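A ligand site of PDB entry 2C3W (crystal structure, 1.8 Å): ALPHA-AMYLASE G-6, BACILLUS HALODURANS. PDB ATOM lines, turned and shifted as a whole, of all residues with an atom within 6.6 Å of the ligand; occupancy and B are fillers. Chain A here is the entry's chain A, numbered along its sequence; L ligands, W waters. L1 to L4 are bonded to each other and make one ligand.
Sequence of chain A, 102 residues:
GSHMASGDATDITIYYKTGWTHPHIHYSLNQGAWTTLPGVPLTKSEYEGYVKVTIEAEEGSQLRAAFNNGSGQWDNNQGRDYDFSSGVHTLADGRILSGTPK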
ATOM      1  N   TYR A  16      -5.755  35.843 -17.564  1.00  0.00           N
ATOM      2  CA  TYR A  16      -6.402  34.557 -17.599  1.00  0.00           C
ATOM      3  C   TYR A  16      -7.159  34.364 -18.877  1.00  0.00           C
ATOM      4  O   TYR A  16      -8.043  35.126 -19.205  1.00  0.00           O
ATOM      5  CB  TYR A  16      -7.401  34.460 -16.435  1.00  0.00           C
ATOM      6  CG  TYR A  16      -8.171  33.160 -16.331  1.00  0.00           C
ATOM      7  CD1 TYR A  16      -7.522  31.939 -16.369  1.00  0.00           C
ATOM      8  CD2 TYR A  16      -9.545  33.172 -16.161  1.00  0.00           C
ATOM      9  CE1 TYR A  16      -8.257  30.769 -16.274  1.00  0.00           C
ATOM     10  CE2 TYR A  16     -10.284  32.010 -15.993  1.00  0.00           C
ATOM     11  CZ  TYR A  16      -9.610  30.814 -16.082  1.00  0.00           C
ATOM     12  OH  TYR A  16     -10.291  29.635 -15.926  1.00  0.00           O
ATOM     13  N   LYS A  17      -6.814  33.315 -19.603  1.00  0.00           N
ATOM     14  CA  LYS A  17      -7.494  32.987 -20.870  1.00  0.00           C
ATOM     15  C   LYS A  17      -8.841  32.345 -20.529  1.00  0.00           C
ATOM     16  O   LYS A  17      -8.881  31.265 -19.945  1.00  0.00           O
ATOM     17  CB  LYS A  17      -6.737  31.961 -21.641  1.00  0.00           C
ATOM     18  CG  LYS A  17      -7.367  31.638 -22.963  1.00  0.00           C
ATOM     19  CD  LYS A  17      -6.512  30.620 -23.693  1.00  0.00           C
ATOM     20  CE  LYS A  17      -7.251  29.886 -24.788  1.00  0.00           C
ATOM     21  NZ  LYS A  17      -6.254  28.958 -25.505  1.00  0.00           N
ATOM     22  N   THR A  18      -9.902  33.020 -20.876  1.00  0.00           N
ATOM     23  CA  THR A  18     -11.244  32.451 -20.748  1.00  0.00           C
ATOM     24  C   THR A  18     -12.252  33.142 -21.610  1.00  0.00           C
ATOM     25  O   THR A  18     -12.104  34.343 -21.938  1.00  0.00           O
ATOM     26  CB  THR A  18     -11.675  32.575 -19.266  1.00  0.00           C
ATOM     27  OG1 THR A  18     -12.943  31.912 -19.058  1.00  0.00           O
ATOM     28  CG2 THR A  18     -11.879  34.022 -18.878  1.00  0.00           C
ATOM     29  N   GLY A  19     -13.307  32.407 -22.000  1.00  0.00           N
ATOM     30  CA  GLY A  19     -14.472  32.976 -22.637  1.00  0.00           C
ATOM     31  C   GLY A  19     -15.648  33.223 -21.694  1.00  0.00           C
ATOM     32  O   GLY A  19     -16.672  33.816 -22.071  1.00  0.00           O
ATOM     33  N   TRP A  20     -15.494  32.833 -20.424  1.00  0.00           N
ATOM     34  CA  TRP A  20     -16.475  33.139 -19.445  1.00  0.00           C
ATOM     35  C   TRP A  20     -16.698  34.647 -19.416  1.00  0.00           C
ATOM     36  O   TRP A  20     -15.722  35.440 -19.447  1.00  0.00           O
ATOM     37  CB  TRP A  20     -15.969  32.698 -18.061  1.00  0.00           C
ATOM     38  CG  TRP A  20     -15.922  31.232 -17.849  1.00  0.00           C
ATOM     39  CD1 TRP A  20     -16.626  30.267 -18.550  1.00  0.00           C
ATOM     40  CD2 TRP A  20     -15.175  30.539 -16.865  1.00  0.00           C
ATOM     41  NE1 TRP A  20     -16.344  29.025 -18.031  1.00  0.00           N
ATOM     42  CE2 TRP A  20     -15.491  29.154 -16.976  1.00  0.00           C
ATOM     43  CE3 TRP A  20     -14.289  30.941 -15.852  1.00  0.00           C
ATOM     44  CZ2 TRP A  20     -14.913  28.189 -16.162  1.00  0.00           C
ATOM     45  CZ3 TRP A  20     -13.719  29.980 -15.034  1.00  0.00           C
ATOM     46  CH2 TRP A  20     -14.030  28.607 -15.204  1.00  0.00           C
ATOM     47  N   GLY A  49      -9.670  37.496 -25.552  1.00  0.00           N
ATOM     48  CA  GLY A  49      -9.648  36.158 -24.989  1.00  0.00           C
ATOM     49  C   GLY A  49      -9.079  36.035 -23.586  1.00  0.00           C
ATOM     50  O   GLY A  49      -9.032  34.943 -23.059  1.00  0.00           O
ATOM     51  N   PHE A  67     -10.341  29.467 -10.297  1.00  0.00           N
ATOM     52  CA  PHE A  67     -11.171  30.346 -11.089  1.00  0.00           C
ATOM     53  C   PHE A  67     -12.546  29.786 -11.273  1.00  0.00           C
ATOM     54  O   PHE A  67     -12.745  28.577 -11.312  1.00  0.00           O
ATOM     55  CB  PHE A  67     -10.485  30.593 -12.425  1.00  0.00           C
ATOM     56  CG  PHE A  67      -9.153  31.288 -12.284  1.00  0.00           C
ATOM     57  CD1 PHE A  67      -9.068  32.667 -12.328  1.00  0.00           C
ATOM     58  CD2 PHE A  67      -7.985  30.569 -12.000  1.00  0.00           C
ATOM     59  CE1 PHE A  67      -7.809  33.327 -12.165  1.00  0.00           C
ATOM     60  CE2 PHE A  67      -6.778  31.192 -11.816  1.00  0.00           C
ATOM     61  CZ  PHE A  67      -6.693  32.615 -11.906  1.00  0.00           C
ATOM     62  N   TRP A  74     -15.990  25.767 -12.438  1.00  0.00           N
ATOM     63  CA  TRP A  74     -14.621  25.974 -11.939  1.00  0.00           C
ATOM     64  C   TRP A  74     -13.477  25.557 -12.880  1.00  0.00           C
ATOM     65  O   TRP A  74     -13.575  24.652 -13.727  1.00  0.00           O
ATOM     66  CB  TRP A  74     -14.424  25.262 -10.584  1.00  0.00           C
ATOM     67  CG  TRP A  74     -15.302  25.856  -9.506  1.00  0.00           C
ATOM     68  CD1 TRP A  74     -16.589  25.566  -9.248  1.00  0.00           C
ATOM     69  CD2 TRP A  74     -14.910  26.872  -8.567  1.00  0.00           C
ATOM     70  NE1 TRP A  74     -17.033  26.325  -8.184  1.00  0.00           N
ATOM     71  CE2 TRP A  74     -16.016  27.134  -7.759  1.00  0.00           C
ATOM     72  CE3 TRP A  74     -13.726  27.557  -8.325  1.00  0.00           C
ATOM     73  CZ2 TRP A  74     -15.970  28.076  -6.725  1.00  0.00           C
ATOM     74  CZ3 TRP A  74     -13.667  28.479  -7.301  1.00  0.00           C
ATOM     75  CH2 TRP A  74     -14.786  28.759  -6.545  1.00  0.00           C
ATOM     76  N   ASP A  75     -12.346  26.229 -12.676  1.00  0.00           N
ATOM     77  CA  ASP A  75     -11.077  25.889 -13.213  1.00  0.00           C
ATOM     78  C   ASP A  75     -10.092  25.850 -12.086  1.00  0.00           C
ATOM     79  O   ASP A  75      -9.610  26.900 -11.641  1.00  0.00           O
ATOM     80  CB  ASP A  75     -10.678  26.876 -14.290  1.00  0.00           C
ATOM     81  CG  ASP A  75      -9.285  26.633 -14.807  1.00  0.00           C
ATOM     82  OD1 ASP A  75      -8.622  25.576 -14.583  1.00  0.00           O
ATOM     83  OD2 ASP A  75      -8.758  27.512 -15.554  1.00  0.00           O
ATOM     84  N   ASN A  76      -9.834  24.658 -11.529  1.00  0.00           N
ATOM     85  CA  ASN A  76      -9.038  24.554 -10.327  1.00  0.00           C
ATOM     86  C   ASN A  76      -7.764  23.693 -10.433  1.00  0.00           C
ATOM     87  O   ASN A  76      -7.245  23.195  -9.441  1.00  0.00           O
ATOM     88  CB  ASN A  76      -9.901  24.057  -9.205  1.00  0.00           C
ATOM     89  CG  ASN A  76     -10.432  22.642  -9.467  1.00  0.00           C
ATOM     90  OD1 ASN A  76      -9.921  21.935 -10.344  1.00  0.00           O
ATOM     91  ND2 ASN A  76     -11.435  22.217  -8.701  1.00  0.00           N
ATOM     92  N   ASN A  77      -7.255  23.539 -11.645  1.00  0.00           N
ATOM     93  CA  ASN A  77      -5.978  22.868 -11.847  1.00  0.00           C
ATOM     94  C   ASN A  77      -5.981  21.416 -11.326  1.00  0.00           C
ATOM     95  O   ASN A  77      -5.119  21.048 -10.555  1.00  0.00           O
ATOM     96  CB  ASN A  77      -4.781  23.602 -11.199  1.00  0.00           C
ATOM     97  CG  ASN A  77      -3.434  23.169 -11.733  1.00  0.00           C
ATOM     98  OD1 ASN A  77      -3.369  22.638 -12.833  1.00  0.00           O
ATOM     99  ND2 ASN A  77      -2.339  23.358 -10.944  1.00  0.00           N
ATOM    100  N   GLN A  78      -6.988  20.660 -11.720  1.00  0.00           N
ATOM    101  CA  GLN A  78      -7.119  19.233 -11.352  1.00  0.00           C
ATOM    102  C   GLN A  78      -7.253  19.119  -9.832  1.00  0.00           C
ATOM    103  O   GLN A  78      -6.793  18.153  -9.213  1.00  0.00           O
ATOM    104  CB  GLN A  78      -5.948  18.372 -11.826  1.00  0.00           C
ATOM    105  CG  GLN A  78      -5.531  18.624 -13.250  1.00  0.00           C
ATOM    106  CD  GLN A  78      -6.644  18.521 -14.296  1.00  0.00           C
ATOM    107  OE1 GLN A  78      -7.580  17.745 -14.145  1.00  0.00           O
ATOM    108  NE2 GLN A  78      -6.515  19.318 -15.414  1.00  0.00           N
ATOM    109  N   TYR A  82      -4.133  26.942  -8.453  1.00  0.00           N
ATOM    110  CA  TYR A  82      -3.052  27.564  -9.122  1.00  0.00           C
ATOM    111  C   TYR A  82      -2.290  28.475  -8.178  1.00  0.00           C
ATOM    112  O   TYR A  82      -2.901  29.231  -7.406  1.00  0.00           O
ATOM    113  CB  TYR A  82      -3.601  28.424 -10.264  1.00  0.00           C
ATOM    114  CG  TYR A  82      -4.255  27.609 -11.354  1.00  0.00           C
ATOM    115  CD1 TYR A  82      -3.476  26.961 -12.274  1.00  0.00           C
ATOM    116  CD2 TYR A  82      -5.643  27.588 -11.523  1.00  0.00           C
ATOM    117  CE1 TYR A  82      -4.052  26.283 -13.327  1.00  0.00           C
ATOM    118  CE2 TYR A  82      -6.241  26.904 -12.534  1.00  0.00           C
ATOM    119  CZ  TYR A  82      -5.416  26.204 -13.430  1.00  0.00           C
ATOM    120  OH  TYR A  82      -5.959  25.529 -14.489  1.00  0.00           O
ATOM    121  N   ALA A  92      -2.989  30.195 -19.144  1.00  0.00           N
ATOM    122  CA  ALA A  92      -3.708  29.745 -20.329  1.00  0.00           C
ATOM    123  C   ALA A  92      -3.693  28.243 -20.406  1.00  0.00           C
ATOM    124  O   ALA A  92      -2.612  27.602 -20.312  1.00  0.00           O
ATOM    125  CB  ALA A  92      -3.011  30.329 -21.588  1.00  0.00           C
ATOM    126  N   ASP A  93      -4.880  27.667 -20.463  1.00  0.00           N
ATOM    127  CA  ASP A  93      -5.061  26.229 -20.587  1.00  0.00           C
ATOM    128  C   ASP A  93      -4.307  25.437 -19.570  1.00  0.00           C
ATOM    129  O   ASP A  93      -3.654  24.389 -19.870  1.00  0.00           O
ATOM    130  CB  ASP A  93      -4.716  25.727 -21.997  1.00  0.00           C
ATOM    131  CG  ASP A  93      -5.464  26.441 -23.066  1.00  0.00           C
ATOM    132  OD1 ASP A  93      -6.676  26.674 -22.934  1.00  0.00           O
ATOM    133  OD2 ASP A  93      -4.893  26.774 -24.130  1.00  0.00           O
ATOM    134  N   GLY A  94      -4.413  25.885 -18.343  1.00  0.00           N
ATOM    135  CA  GLY A  94      -3.831  25.233 -17.236  1.00  0.00           C
ATOM    136  C   GLY A  94      -2.344  25.449 -17.007  1.00  0.00           C
ATOM    137  O   GLY A  94      -1.824  24.856 -16.095  1.00  0.00           O
ATOM    138  N   ARG A  95      -1.682  26.317 -17.774  1.00  0.00           N
ATOM    139  CA  ARG A  95      -0.274  26.534 -17.665  1.00  0.00           C
ATOM    140  C   ARG A  95      -0.001  27.975 -17.332  1.00  0.00           C
ATOM    141  O   ARG A  95      -0.539  28.859 -17.954  1.00  0.00           O
ATOM    142  CB  ARG A  95       0.397  26.245 -19.002  1.00  0.00           C
ATOM    143  CG  ARG A  95       0.079  24.869 -19.554  1.00  0.00           C
ATOM    144  CD  ARG A  95       1.223  24.259 -20.387  1.00  0.00           C
ATOM    145  NE  ARG A  95       2.070  25.306 -20.997  1.00  0.00           N
ATOM    146  CZ  ARG A  95       3.089  25.964 -20.410  1.00  0.00           C
ATOM    147  NH1 ARG A  95       3.477  25.710 -19.140  1.00  0.00           N
ATOM    148  NH2 ARG A  95       3.725  26.888 -21.090  1.00  0.00           N
HETATM  149  C1  LIG L   1      -6.804  23.117 -18.322  1.00  0.00           C
HETATM  150  C2  LIG L   1      -7.628  23.259 -17.000  1.00  0.00           C
HETATM  151  C3  LIG L   1      -9.136  23.387 -17.187  1.00  0.00           C
HETATM  152  C4  LIG L   1      -9.398  24.548 -18.177  1.00  0.00           C
HETATM  153  C5  LIG L   1      -8.562  24.269 -19.449  1.00  0.00           C
HETATM  154  C6  LIG L   1      -8.753  25.311 -20.521  1.00  0.00           C
HETATM  155  O1  LIG L   1      -7.122  21.895 -18.913  1.00  0.00           O
HETATM  156  O2  LIG L   1      -7.202  22.237 -16.047  1.00  0.00           O
HETATM  157  O3  LIG L   1      -9.761  23.632 -15.954  1.00  0.00           O
HETATM  158  O4  LIG L   1     -10.716  24.579 -18.636  1.00  0.00           O
HETATM  159  O5  LIG L   1      -7.187  24.125 -19.205  1.00  0.00           O
HETATM  160  O6  LIG L   1      -8.114  24.814 -21.700  1.00  0.00           O
HETATM  161  C1  LG2 L   2     -11.572  25.362 -17.727  1.00  0.00           C
HETATM  162  C2  LG2 L   2     -13.020  25.007 -17.983  1.00  0.00           C
HETATM  163  C3  LG2 L   2     -13.415  25.532 -19.371  1.00  0.00           C
HETATM  164  C4  LG2 L   2     -13.074  27.023 -19.452  1.00  0.00           C
HETATM  165  C5  LG2 L   2     -11.630  27.313 -19.048  1.00  0.00           C
HETATM  166  C6  LG2 L   2     -11.235  28.777 -19.021  1.00  0.00           C
HETATM  167  O1  LG2 L   2     -13.111  23.616 -17.880  1.00  0.00           O
HETATM  168  O2  LG2 L   2     -14.787  25.459 -19.622  1.00  0.00           O
HETATM  169  O3  LG2 L   2     -13.222  27.414 -20.800  1.00  0.00           O
HETATM  170  O4  LG2 L   2     -11.265  26.756 -17.802  1.00  0.00           O
HETATM  171  O5  LG2 L   2     -12.078  29.451 -18.115  1.00  0.00           O
HETATM  172  C1  LG3 L   3     -13.971  28.609 -21.031  1.00  0.00           C
HETATM  173  C2  LG3 L   3     -15.303  28.260 -21.682  1.00  0.00           C
HETATM  174  C3  LG3 L   3     -15.049  27.678 -23.075  1.00  0.00           C
HETATM  175  C4  LG3 L   3     -14.124  28.568 -23.890  1.00  0.00           C
HETATM  176  C5  LG3 L   3     -12.826  28.900 -23.099  1.00  0.00           C
HETATM  177  C6  LG3 L   3     -12.071  30.003 -23.860  1.00  0.00           C
HETATM  178  O1  LG3 L   3     -16.093  27.358 -20.888  1.00  0.00           O
HETATM  179  O2  LG3 L   3     -16.330  27.564 -23.709  1.00  0.00           O
HETATM  180  O3  LG3 L   3     -13.810  27.861 -25.081  1.00  0.00           O
HETATM  181  O4  LG3 L   3     -13.231  29.482 -21.869  1.00  0.00           O
HETATM  182  O5  LG3 L   3     -10.881  30.354 -23.168  1.00  0.00           O
HETATM  183  C1  LG4 L   4     -14.696  28.147 -26.198  1.00  0.00           C
HETATM  184  C2  LG4 L   4     -14.879  26.810 -26.945  1.00  0.00           C
HETATM  185  C3  LG4 L   4     -13.596  26.281 -27.521  1.00  0.00           C
HETATM  186  C4  LG4 L   4     -13.135  27.348 -28.486  1.00  0.00           C
HETATM  187  C5  LG4 L   4     -12.992  28.683 -27.752  1.00  0.00           C
HETATM  188  C6  LG4 L   4     -12.432  29.699 -28.735  1.00  0.00           C
HETATM  189  O1  LG4 L   4     -15.363  25.800 -26.071  1.00  0.00           O
HETATM  190  O2  LG4 L   4     -13.809  25.050 -28.217  1.00  0.00           O
HETATM  191  O3  LG4 L   4     -11.883  26.939 -28.966  1.00  0.00           O
HETATM  192  O4  LG4 L   4     -14.213  29.138 -27.086  1.00  0.00           O
HETATM  193  O5  LG4 L   4     -12.749  30.929 -28.151  1.00  0.00           O
HETATM  194  O   HOH W   1      -9.312  28.312 -21.992  1.00  0.00           O
HETATM  195  O   HOH W   2     -16.992  25.782 -17.747  1.00  0.00           O
HETATM  196  O   HOH W   3     -18.109  25.706 -22.508  1.00  0.00           O
HETATM  197  O   HOH W   4     -10.249  32.840 -24.382  1.00  0.00           O
HETATM  198  O   HOH W   5     -14.434  32.017 -26.462  1.00  0.00           O
HETATM  199  O   HOH W   6     -15.153  23.841 -15.648  1.00  0.00           O
HETATM  200  O   HOH W   7     -13.977  22.374 -27.234  1.00  0.00           O
HETATM  201  O   HOH W   8     -17.677  29.838 -24.349  1.00  0.00           O
HETATM  202  O   HOH W   9     -18.935  28.662 -20.790  1.00  0.00           O
HETATM  203  O   HOH W  10      -9.700  30.442 -27.420  1.00  0.00           O
HETATM  204  O   HOH W  11      -4.626  21.797 -15.171  1.00  0.00           O
HETATM  205  O   HOH W  12     -18.764  25.713 -20.076  1.00  0.00           O
HETATM  206  O   HOH W  13      -8.775  21.509 -13.946  1.00  0.00           O
HETATM  207  O   HOH W  14     -13.276  24.367 -23.714  1.00  0.00           O
HETATM  208  O   HOH W  15      -6.258  22.067 -21.639  1.00  0.00           O
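The side-chain hydroxyl (OG1) of Thr 18 sits at hydrogen-bond distance from an oxygen (O5) of LG2 L2 (2.8 Å). OH of Tyr 16 sits at hydrogen-bond distance from O5 of LG2 L2, 2.8 Å away. N of Gly 94 is in hydrogen-bond range of O5 of LIG L1. The indole nitrogen (NE1) of Trp 20 is in hydrogen-bond range of an oxygen (O1) of LG3 L3 (3.3 Å). The side-chain amide nitrogen (NE2) of Gln 78 is in hydrogen-bond range of an oxygen (O2) of LIG L1 (3.1 Å). An oxygen (O3) of LIG L1 lies within hydrogen-bond range of the side-chain carboxylate of Asp 75 (2.6 Å). The backbone NH (N) of Gly 19 is in hydrogen-bond range of an oxygen (O4) of LG3 L3 (2.9 Å). OD1 of Asp 93 lies within hydrogen-bond range of O6 of LIG L1 (2.7 Å).
The backbone NH (N) of Gln 78 sits close to the side-chain amide oxygen (OD1) of Asn 76 (3.5 Å). OH of Tyr 16 is in hydrogen-bond range of OD2 of Asp 75, at 2.6 Å. The backbone NH of Trp 20 is in hydrogen-bond range of the side-chain hydroxyl of Thr 18, 3.0 Å away. The side-chain amino group of Lys 17 lies within salt-bridge range of the side-chain carboxylate of Asp 93, 2.9 Å away. O of Gly 49 sits at hydrogen-bond distance from N of Thr 18, 3.0 Å away. The backbone NH (N) of Asp 75 is in hydrogen-bond range of the backbone carbonyl oxygen (O) of Phe 67. The side-chain hydroxyl (OH) of Tyr 82 lies within hydrogen-bond range of the side-chain carboxylate (OD1) of Asp 75 (2.7 Å).
Merely in contact with the ligand: Lys 17 (3.5 Å) and Tyr 82 (3.8 Å). Of the 17 residues printed, 10 come within 4 Å of the ligand.
Water W13 lies within hydrogen-bond range of O2 of LIG L1 (2.7 Å), N of Gln 78 (3.0 Å) and N of Asn 77 (3.4 Å). Water W11 lies within hydrogen-bond range of O2 of LIG L1 (2.8 Å), OD1 of Asn 77 (2.8 Å) and NE2 of Gln 78 (3.1 Å). Water W1 bridges an oxygen (O5) of LG3 L3 (2.8 Å) and the side-chain carboxylate (OD1) of Asp 93 (3.2 Å). Water W4 lies within hydrogen-bond range of the backbone carbonyl oxygen of Gly 49, an oxygen (O5) of LG3 L3 and the backbone carbonyl oxygen of Thr 18. Water W2 lies within hydrogen-bond range of an oxygen (O2) of LG2 L2 (2.9 Å) and the indole nitrogen of Trp 20 (3.3 Å). Water W6 bridges the backbone carbonyl oxygen of Trp 74 and an oxygen (O1) of LG2 L2.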
